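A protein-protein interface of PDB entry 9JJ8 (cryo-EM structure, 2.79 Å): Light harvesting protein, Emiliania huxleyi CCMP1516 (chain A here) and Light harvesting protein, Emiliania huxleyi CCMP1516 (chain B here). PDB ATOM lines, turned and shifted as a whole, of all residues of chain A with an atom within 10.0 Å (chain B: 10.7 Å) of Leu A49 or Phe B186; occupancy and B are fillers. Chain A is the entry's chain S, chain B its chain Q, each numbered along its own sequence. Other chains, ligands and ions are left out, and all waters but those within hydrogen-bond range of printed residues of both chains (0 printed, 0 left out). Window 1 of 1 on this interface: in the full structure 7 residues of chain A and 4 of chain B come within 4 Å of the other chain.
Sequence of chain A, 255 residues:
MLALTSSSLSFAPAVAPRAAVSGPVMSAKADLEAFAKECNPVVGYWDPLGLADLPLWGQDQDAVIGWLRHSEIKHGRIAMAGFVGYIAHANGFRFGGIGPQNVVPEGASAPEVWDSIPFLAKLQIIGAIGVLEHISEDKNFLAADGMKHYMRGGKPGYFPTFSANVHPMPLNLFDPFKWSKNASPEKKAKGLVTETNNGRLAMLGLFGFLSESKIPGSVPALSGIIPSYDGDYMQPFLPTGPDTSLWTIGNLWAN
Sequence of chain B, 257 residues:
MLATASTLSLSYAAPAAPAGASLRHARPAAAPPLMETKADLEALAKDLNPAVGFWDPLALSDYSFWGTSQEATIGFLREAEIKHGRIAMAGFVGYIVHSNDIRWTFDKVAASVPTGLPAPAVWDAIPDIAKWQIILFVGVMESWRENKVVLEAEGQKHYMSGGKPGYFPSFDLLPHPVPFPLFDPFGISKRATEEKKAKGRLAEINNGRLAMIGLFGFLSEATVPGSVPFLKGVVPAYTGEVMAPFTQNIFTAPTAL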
ATOM      1  N   LYS A  29      26.487  24.028 -11.501  1.00  0.00           N
ATOM      2  CA  LYS A  29      26.893  24.389 -10.150  1.00  0.00           C
ATOM      3  C   LYS A  29      28.399  24.263  -9.971  1.00  0.00           C
ATOM      4  O   LYS A  29      28.982  25.012  -9.189  1.00  0.00           O
ATOM      5  CB  LYS A  29      26.144  23.529  -9.129  1.00  0.00           C
ATOM      6  CG  LYS A  29      26.349  23.948  -7.676  1.00  0.00           C
ATOM      7  CD  LYS A  29      25.443  23.176  -6.734  1.00  0.00           C
ATOM      8  CE  LYS A  29      24.039  23.754  -6.723  1.00  0.00           C
ATOM      9  NZ  LYS A  29      24.016  25.155  -6.213  1.00  0.00           N
ATOM     10  N   TYR A  45      31.804  29.967  -2.382  1.00  0.00           N
ATOM     11  CA  TYR A  45      30.402  29.958  -2.782  1.00  0.00           C
ATOM     12  C   TYR A  45      29.533  30.413  -1.619  1.00  0.00           C
ATOM     13  O   TYR A  45      29.428  29.718  -0.604  1.00  0.00           O
ATOM     14  CB  TYR A  45      30.001  28.560  -3.241  1.00  0.00           C
ATOM     15  CG  TYR A  45      28.574  28.444  -3.719  1.00  0.00           C
ATOM     16  CD1 TYR A  45      28.188  28.970  -4.943  1.00  0.00           C
ATOM     17  CD2 TYR A  45      27.614  27.792  -2.953  1.00  0.00           C
ATOM     18  CE1 TYR A  45      26.887  28.860  -5.390  1.00  0.00           C
ATOM     19  CE2 TYR A  45      26.308  27.674  -3.395  1.00  0.00           C
ATOM     20  CZ  TYR A  45      25.952  28.210  -4.615  1.00  0.00           C
ATOM     21  OH  TYR A  45      24.655  28.102  -5.062  1.00  0.00           O
ATOM     22  N   TRP A  46      28.904  31.575  -1.761  1.00  0.00           N
ATOM     23  CA  TRP A  46      27.998  32.106  -0.746  1.00  0.00           C
ATOM     24  C   TRP A  46      26.616  32.283  -1.366  1.00  0.00           C
ATOM     25  O   TRP A  46      26.358  33.276  -2.052  1.00  0.00           O
ATOM     26  CB  TRP A  46      28.512  33.419  -0.168  1.00  0.00           C
ATOM     27  CG  TRP A  46      27.701  33.853   0.999  1.00  0.00           C
ATOM     28  CD1 TRP A  46      26.839  34.907   1.053  1.00  0.00           C
ATOM     29  CD2 TRP A  46      27.643  33.218   2.280  1.00  0.00           C
ATOM     30  NE1 TRP A  46      26.258  34.978   2.296  1.00  0.00           N
ATOM     31  CE2 TRP A  46      26.735  33.951   3.068  1.00  0.00           C
ATOM     32  CE3 TRP A  46      28.278  32.105   2.841  1.00  0.00           C
ATOM     33  CZ2 TRP A  46      26.442  33.603   4.384  1.00  0.00           C
ATOM     34  CZ3 TRP A  46      27.990  31.766   4.148  1.00  0.00           C
ATOM     35  CH2 TRP A  46      27.083  32.514   4.907  1.00  0.00           C
ATOM     36  N   ASP A  47      25.730  31.321  -1.118  1.00  0.00           N
ATOM     37  CA  ASP A  47      24.335  31.389  -1.551  1.00  0.00           C
ATOM     38  C   ASP A  47      23.435  31.044  -0.372  1.00  0.00           C
ATOM     39  O   ASP A  47      22.952  29.913  -0.252  1.00  0.00           O
ATOM     40  CB  ASP A  47      24.081  30.447  -2.729  1.00  0.00           C
ATOM     41  CG  ASP A  47      22.813  30.788  -3.487  1.00  0.00           C
ATOM     42  OD1 ASP A  47      22.126  31.757  -3.103  1.00  0.00           O
ATOM     43  OD2 ASP A  47      22.503  30.083  -4.469  1.00  0.00           O
ATOM     44  N   PRO A  48      23.202  32.000   0.533  1.00  0.00           N
ATOM     45  CA  PRO A  48      22.301  31.722   1.662  1.00  0.00           C
ATOM     46  C   PRO A  48      20.849  31.574   1.249  1.00  0.00           C
ATOM     47  O   PRO A  48      20.109  30.807   1.878  1.00  0.00           O
ATOM     48  CB  PRO A  48      22.510  32.936   2.577  1.00  0.00           C
ATOM     49  CG  PRO A  48      22.899  34.032   1.648  1.00  0.00           C
ATOM     50  CD  PRO A  48      23.700  33.387   0.550  1.00  0.00           C
ATOM     51  N   LEU A  49      20.416  32.283   0.205  1.00  0.00           N
ATOM     52  CA  LEU A  49      19.046  32.179  -0.277  1.00  0.00           C
ATOM     53  C   LEU A  49      18.818  30.959  -1.159  1.00  0.00           C
ATOM     54  O   LEU A  49      17.667  30.534  -1.310  1.00  0.00           O
ATOM     55  CB  LEU A  49      18.658  33.443  -1.048  1.00  0.00           C
ATOM     56  CG  LEU A  49      17.868  34.510  -0.287  1.00  0.00           C
ATOM     57  CD1 LEU A  49      18.699  35.126   0.828  1.00  0.00           C
ATOM     58  CD2 LEU A  49      17.364  35.583  -1.240  1.00  0.00           C
ATOM     59  N   GLY A  50      19.872  30.390  -1.735  1.00  0.00           N
ATOM     60  CA  GLY A  50      19.723  29.223  -2.590  1.00  0.00           C
ATOM     61  C   GLY A  50      18.963  29.483  -3.872  1.00  0.00           C
ATOM     62  O   GLY A  50      18.221  28.610  -4.338  1.00  0.00           O
ATOM     63  N   LEU A  51      19.135  30.670  -4.461  1.00  0.00           N
ATOM     64  CA  LEU A  51      18.470  30.985  -5.722  1.00  0.00           C
ATOM     65  C   LEU A  51      19.049  30.206  -6.893  1.00  0.00           C
ATOM     66  O   LEU A  51      18.410  30.131  -7.948  1.00  0.00           O
ATOM     67  CB  LEU A  51      18.559  32.484  -6.014  1.00  0.00           C
ATOM     68  CG  LEU A  51      17.777  33.433  -5.112  1.00  0.00           C
ATOM     69  CD1 LEU A  51      17.916  34.863  -5.599  1.00  0.00           C
ATOM     70  CD2 LEU A  51      16.325  33.021  -5.092  1.00  0.00           C
ATOM     71  N   ALA A  52      20.233  29.625  -6.733  1.00  0.00           N
ATOM     72  CA  ALA A  52      20.860  28.814  -7.764  1.00  0.00           C
ATOM     73  C   ALA A  52      20.289  27.406  -7.835  1.00  0.00           C
ATOM     74  O   ALA A  52      20.727  26.619  -8.678  1.00  0.00           O
ATOM     75  CB  ALA A  52      22.368  28.749  -7.533  1.00  0.00           C
ATOM     76  N   ASP A  53      19.344  27.065  -6.960  1.00  0.00           N
ATOM     77  CA  ASP A  53      18.633  25.799  -7.027  1.00  0.00           C
ATOM     78  C   ASP A  53      17.179  25.953  -7.441  1.00  0.00           C
ATOM     79  O   ASP A  53      16.508  24.941  -7.672  1.00  0.00           O
ATOM     80  CB  ASP A  53      18.691  25.078  -5.672  1.00  0.00           C
ATOM     81  CG  ASP A  53      20.074  24.552  -5.353  1.00  0.00           C
ATOM     82  OD1 ASP A  53      20.795  24.173  -6.298  1.00  0.00           O
ATOM     83  OD2 ASP A  53      20.440  24.522  -4.160  1.00  0.00           O
ATOM     84  N   LEU A  54      16.678  27.177  -7.540  1.00  0.00           N
ATOM     85  CA  LEU A  54      15.278  27.407  -7.864  1.00  0.00           C
ATOM     86  C   LEU A  54      15.081  27.396  -9.375  1.00  0.00           C
ATOM     87  O   LEU A  54      15.722  28.184 -10.077  1.00  0.00           O
ATOM     88  CB  LEU A  54      14.825  28.744  -7.293  1.00  0.00           C
ATOM     89  CG  LEU A  54      14.067  28.746  -5.966  1.00  0.00           C
ATOM     90  CD1 LEU A  54      14.956  28.286  -4.828  1.00  0.00           C
ATOM     91  CD2 LEU A  54      13.554  30.139  -5.685  1.00  0.00           C
ATOM     92  N   LEU A  68      21.038  34.304 -13.867  1.00  0.00           N
ATOM     93  CA  LEU A  68      21.529  34.929 -12.641  1.00  0.00           C
ATOM     94  C   LEU A  68      22.874  35.611 -12.864  1.00  0.00           C
ATOM     95  O   LEU A  68      23.084  36.751 -12.429  1.00  0.00           O
ATOM     96  CB  LEU A  68      21.623  33.887 -11.526  1.00  0.00           C
ATOM     97  CG  LEU A  68      20.291  33.458 -10.907  1.00  0.00           C
ATOM     98  CD1 LEU A  68      20.464  32.207 -10.059  1.00  0.00           C
ATOM     99  CD2 LEU A  68      19.688  34.587 -10.088  1.00  0.00           C
ATOM    100  N   PRO B 179       8.429  30.841  -7.324  1.00  0.00           N
ATOM    101  CA  PRO B 179       9.592  30.539  -6.484  1.00  0.00           C
ATOM    102  C   PRO B 179       9.174  30.329  -5.036  1.00  0.00           C
ATOM    103  O   PRO B 179       8.111  30.791  -4.610  1.00  0.00           O
ATOM    104  CB  PRO B 179      10.461  31.792  -6.636  1.00  0.00           C
ATOM    105  CG  PRO B 179       9.475  32.883  -6.905  1.00  0.00           C
ATOM    106  CD  PRO B 179       8.423  32.245  -7.772  1.00  0.00           C
ATOM    107  N   PHE B 180      10.040  29.632  -4.272  1.00  0.00           N
ATOM    108  CA  PHE B 180       9.869  29.455  -2.829  1.00  0.00           C
ATOM    109  C   PHE B 180       8.589  28.745  -2.386  1.00  0.00           C
ATOM    110  O   PHE B 180       7.542  29.388  -2.263  1.00  0.00           O
ATOM    111  CB  PHE B 180       9.959  30.803  -2.106  1.00  0.00           C
ATOM    112  CG  PHE B 180      11.174  31.605  -2.458  1.00  0.00           C
ATOM    113  CD1 PHE B 180      12.441  31.135  -2.151  1.00  0.00           C
ATOM    114  CD2 PHE B 180      11.050  32.839  -3.072  1.00  0.00           C
ATOM    115  CE1 PHE B 180      13.562  31.878  -2.463  1.00  0.00           C
ATOM    116  CE2 PHE B 180      12.165  33.585  -3.387  1.00  0.00           C
ATOM    117  CZ  PHE B 180      13.422  33.105  -3.079  1.00  0.00           C
ATOM    118  N   PRO B 181       8.587  27.423  -2.243  1.00  0.00           N
ATOM    119  CA  PRO B 181       7.522  26.758  -1.474  1.00  0.00           C
ATOM    120  C   PRO B 181       7.528  27.224  -0.013  1.00  0.00           C
ATOM    121  O   PRO B 181       8.411  27.955   0.427  1.00  0.00           O
ATOM    122  CB  PRO B 181       7.885  25.277  -1.585  1.00  0.00           C
ATOM    123  CG  PRO B 181       9.362  25.266  -1.759  1.00  0.00           C
ATOM    124  CD  PRO B 181       9.718  26.518  -2.519  1.00  0.00           C
ATOM    125  N   LEU B 182       6.524  26.779   0.753  1.00  0.00           N
ATOM    126  CA  LEU B 182       6.437  27.199   2.154  1.00  0.00           C
ATOM    127  C   LEU B 182       7.573  26.616   2.984  1.00  0.00           C
ATOM    128  O   LEU B 182       8.340  27.356   3.612  1.00  0.00           O
ATOM    129  CB  LEU B 182       5.094  26.805   2.779  1.00  0.00           C
ATOM    130  CG  LEU B 182       3.760  27.471   2.447  1.00  0.00           C
ATOM    131  CD1 LEU B 182       2.642  26.775   3.207  1.00  0.00           C
ATOM    132  CD2 LEU B 182       3.788  28.933   2.822  1.00  0.00           C
ATOM    133  N   PHE B 183       7.684  25.290   3.013  1.00  0.00           N
ATOM    134  CA  PHE B 183       8.719  24.652   3.815  1.00  0.00           C
ATOM    135  C   PHE B 183      10.089  24.936   3.219  1.00  0.00           C
ATOM    136  O   PHE B 183      10.274  24.829   2.002  1.00  0.00           O
ATOM    137  CB  PHE B 183       8.484  23.147   3.897  1.00  0.00           C
ATOM    138  CG  PHE B 183       9.456  22.439   4.795  1.00  0.00           C
ATOM    139  CD1 PHE B 183       9.767  22.961   6.039  1.00  0.00           C
ATOM    140  CD2 PHE B 183      10.059  21.257   4.397  1.00  0.00           C
ATOM    141  CE1 PHE B 183      10.663  22.321   6.871  1.00  0.00           C
ATOM    142  CE2 PHE B 183      10.955  20.609   5.228  1.00  0.00           C
ATOM    143  CZ  PHE B 183      11.256  21.142   6.467  1.00  0.00           C
ATOM    144  N   ASP B 184      11.027  25.348   4.096  1.00  0.00           N
ATOM    145  CA  ASP B 184      12.427  25.757   3.923  1.00  0.00           C
ATOM    146  C   ASP B 184      12.692  26.367   2.546  1.00  0.00           C
ATOM    147  O   ASP B 184      13.465  25.812   1.755  1.00  0.00           O
ATOM    148  CB  ASP B 184      13.403  24.610   4.271  1.00  0.00           C
ATOM    149  CG  ASP B 184      13.211  23.323   3.456  1.00  0.00           C
ATOM    150  OD1 ASP B 184      12.473  23.275   2.459  1.00  0.00           O
ATOM    151  OD2 ASP B 184      13.835  22.314   3.844  1.00  0.00           O
ATOM    152  N   PRO B 185      12.065  27.511   2.236  1.00  0.00           N
ATOM    153  CA  PRO B 185      12.144  28.058   0.869  1.00  0.00           C
ATOM    154  C   PRO B 185      13.543  28.435   0.429  1.00  0.00           C
ATOM    155  O   PRO B 185      13.857  28.336  -0.763  1.00  0.00           O
ATOM    156  CB  PRO B 185      11.237  29.291   0.939  1.00  0.00           C
ATOM    157  CG  PRO B 185      11.291  29.710   2.348  1.00  0.00           C
ATOM    158  CD  PRO B 185      11.409  28.453   3.160  1.00  0.00           C
ATOM    159  N   PHE B 186      14.393  28.872   1.356  1.00  0.00           N
ATOM    160  CA  PHE B 186      15.775  29.161   1.002  1.00  0.00           C
ATOM    161  C   PHE B 186      16.602  27.888   0.905  1.00  0.00           C
ATOM    162  O   PHE B 186      17.658  27.886   0.263  1.00  0.00           O
ATOM    163  CB  PHE B 186      16.401  30.116   2.021  1.00  0.00           C
ATOM    164  CG  PHE B 186      15.847  31.519   1.978  1.00  0.00           C
ATOM    165  CD1 PHE B 186      15.040  31.945   0.931  1.00  0.00           C
ATOM    166  CD2 PHE B 186      16.147  32.417   2.989  1.00  0.00           C
ATOM    167  CE1 PHE B 186      14.537  33.234   0.903  1.00  0.00           C
ATOM    168  CE2 PHE B 186      15.648  33.706   2.966  1.00  0.00           C
ATOM    169  CZ  PHE B 186      14.843  34.115   1.921  1.00  0.00           C
ATOM    170  N   GLY B 187      16.138  26.806   1.516  1.00  0.00           N
ATOM    171  CA  GLY B 187      16.869  25.564   1.547  1.00  0.00           C
ATOM    172  C   GLY B 187      17.681  25.327   2.797  1.00  0.00           C
ATOM    173  O   GLY B 187      18.779  24.766   2.701  1.00  0.00           O
ATOM    174  N   ILE B 188      17.182  25.740   3.967  1.00  0.00           N
ATOM    175  CA  ILE B 188      17.955  25.628   5.202  1.00  0.00           C
ATOM    176  C   ILE B 188      18.102  24.170   5.628  1.00  0.00           C
ATOM    177  O   ILE B 188      19.055  23.812   6.331  1.00  0.00           O
ATOM    178  CB  ILE B 188      17.307  26.501   6.303  1.00  0.00           C
ATOM    179  CG1 ILE B 188      18.254  26.688   7.493  1.00  0.00           C
ATOM    180  CG2 ILE B 188      15.964  25.932   6.751  1.00  0.00           C
ATOM    181  CD1 ILE B 188      17.710  27.608   8.565  1.00  0.00           C
ATOM    182  N   SER B 189      17.194  23.302   5.188  1.00  0.00           N
ATOM    183  CA  SER B 189      17.220  21.890   5.545  1.00  0.00           C
ATOM    184  C   SER B 189      17.074  21.018   4.307  1.00  0.00           C
ATOM    185  O   SER B 189      16.404  19.981   4.332  1.00  0.00           O
ATOM    186  CB  SER B 189      16.132  21.565   6.566  1.00  0.00           C
ATOM    187  OG  SER B 189      14.845  21.856   6.050  1.00  0.00           O
ATOM    188  N   LYS B 190      17.686  21.439   3.196  1.00  0.00           N
ATOM    189  CA  LYS B 190      17.713  20.599   2.002  1.00  0.00           C
ATOM    190  C   LYS B 190      18.526  19.335   2.244  1.00  0.00           C
ATOM    191  O   LYS B 190      18.139  18.242   1.818  1.00  0.00           O
ATOM    192  CB  LYS B 190      18.269  21.383   0.813  1.00  0.00           C
ATOM    193  CG  LYS B 190      17.226  22.208   0.081  1.00  0.00           C
ATOM    194  CD  LYS B 190      16.102  21.327  -0.445  1.00  0.00           C
ATOM    195  CE  LYS B 190      15.039  22.147  -1.156  1.00  0.00           C
ATOM    196  NZ  LYS B 190      15.576  22.815  -2.373  1.00  0.00           N
ATOM    197  N   ARG B 191      19.658  19.466   2.928  1.00  0.00           N
ATOM    198  CA  ARG B 191      20.413  18.314   3.398  1.00  0.00           C
ATOM    199  C   ARG B 191      20.237  18.203   4.909  1.00  0.00           C
ATOM    200  O   ARG B 191      20.341  19.201   5.633  1.00  0.00           O
ATOM    201  CB  ARG B 191      21.892  18.398   2.980  1.00  0.00           C
ATOM    202  CG  ARG B 191      22.848  19.256   3.819  1.00  0.00           C
ATOM    203  CD  ARG B 191      22.670  20.746   3.557  1.00  0.00           C
ATOM    204  NE  ARG B 191      23.598  21.556   4.338  1.00  0.00           N
ATOM    205  CZ  ARG B 191      23.420  21.887   5.610  1.00  0.00           C
ATOM    206  NH1 ARG B 191      22.350  21.499   6.284  1.00  0.00           N
ATOM    207  NH2 ARG B 191      24.339  22.631   6.221  1.00  0.00           N
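The backbone carbonyl oxygen (O) of Phe B186 lies close to the backbone carbonyl oxygen (O) of Leu A49, at 3.1 Å.
The side-chain carboxylate of Asp A47 lies within hydrogen-bond range of the backbone NH of Leu A51 (3.4 Å).
The side-chain carboxylate (OD1) of Asp A47 sits at hydrogen-bond distance from the backbone NH (N) of Gly A50, at 3.0 Å.
Among the printed residues, merely in contact across the chains: Pro A48 with Phe B186 (3.8 Å), Gly A50 with Phe B186 (3.8 Å), Leu A51 with Phe B180 (3.5 Å), Leu A54 with Pro B179 (3.6 Å) and Leu A54 with Phe B180 (3.7 Å).
No residue of chain B comes within 4 Å of Asp A47.
Of the printed residues of chain B, Pro A48 touches Phe B186.
Leu A49 touches one residue of chain B.
Gly A50 touches one residue of chain B.
Of the printed residues of chain B, Leu A51 touches Phe B180.
Printed residues of chain B within 4 Å of Leu A54: Pro B179 (3.6 Å) and Phe B180 (3.7 Å).
Of the printed residues of chain A, Pro B179 touches Leu A54.
Of the printed residues of chain A, Phe B180 touches Leu A51 (3.5 Å) and Leu A54 (3.7 Å).
Asp B184 touches none of the printed residues of chain A.
No residue of chain A comes within 4 Å of Pro B185.
Phe B186 touches just these residues of chain A: Pro A48 (3.8 Å), Leu A49 (3.1 Å) and Gly A50 (3.8 Å).
No residue of chain A comes within 4 Å of Gly B187.
The nearest printed residue of chain B that does not touch Leu A54 is Pro B185 (4.2 Å).
Hydrophobic or aromatic side chains of chain A within 4 Å of the printed part of chain B: Leu A49, Leu A51 and Leu A54.
Of the 13 printed residues of chain B, 3 touch a printed residue of chain A.
Hydrophobic or aromatic side chains of chain B within 4 Å of the printed part of chain A: Pro B179, Phe B180 and Phe B186.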
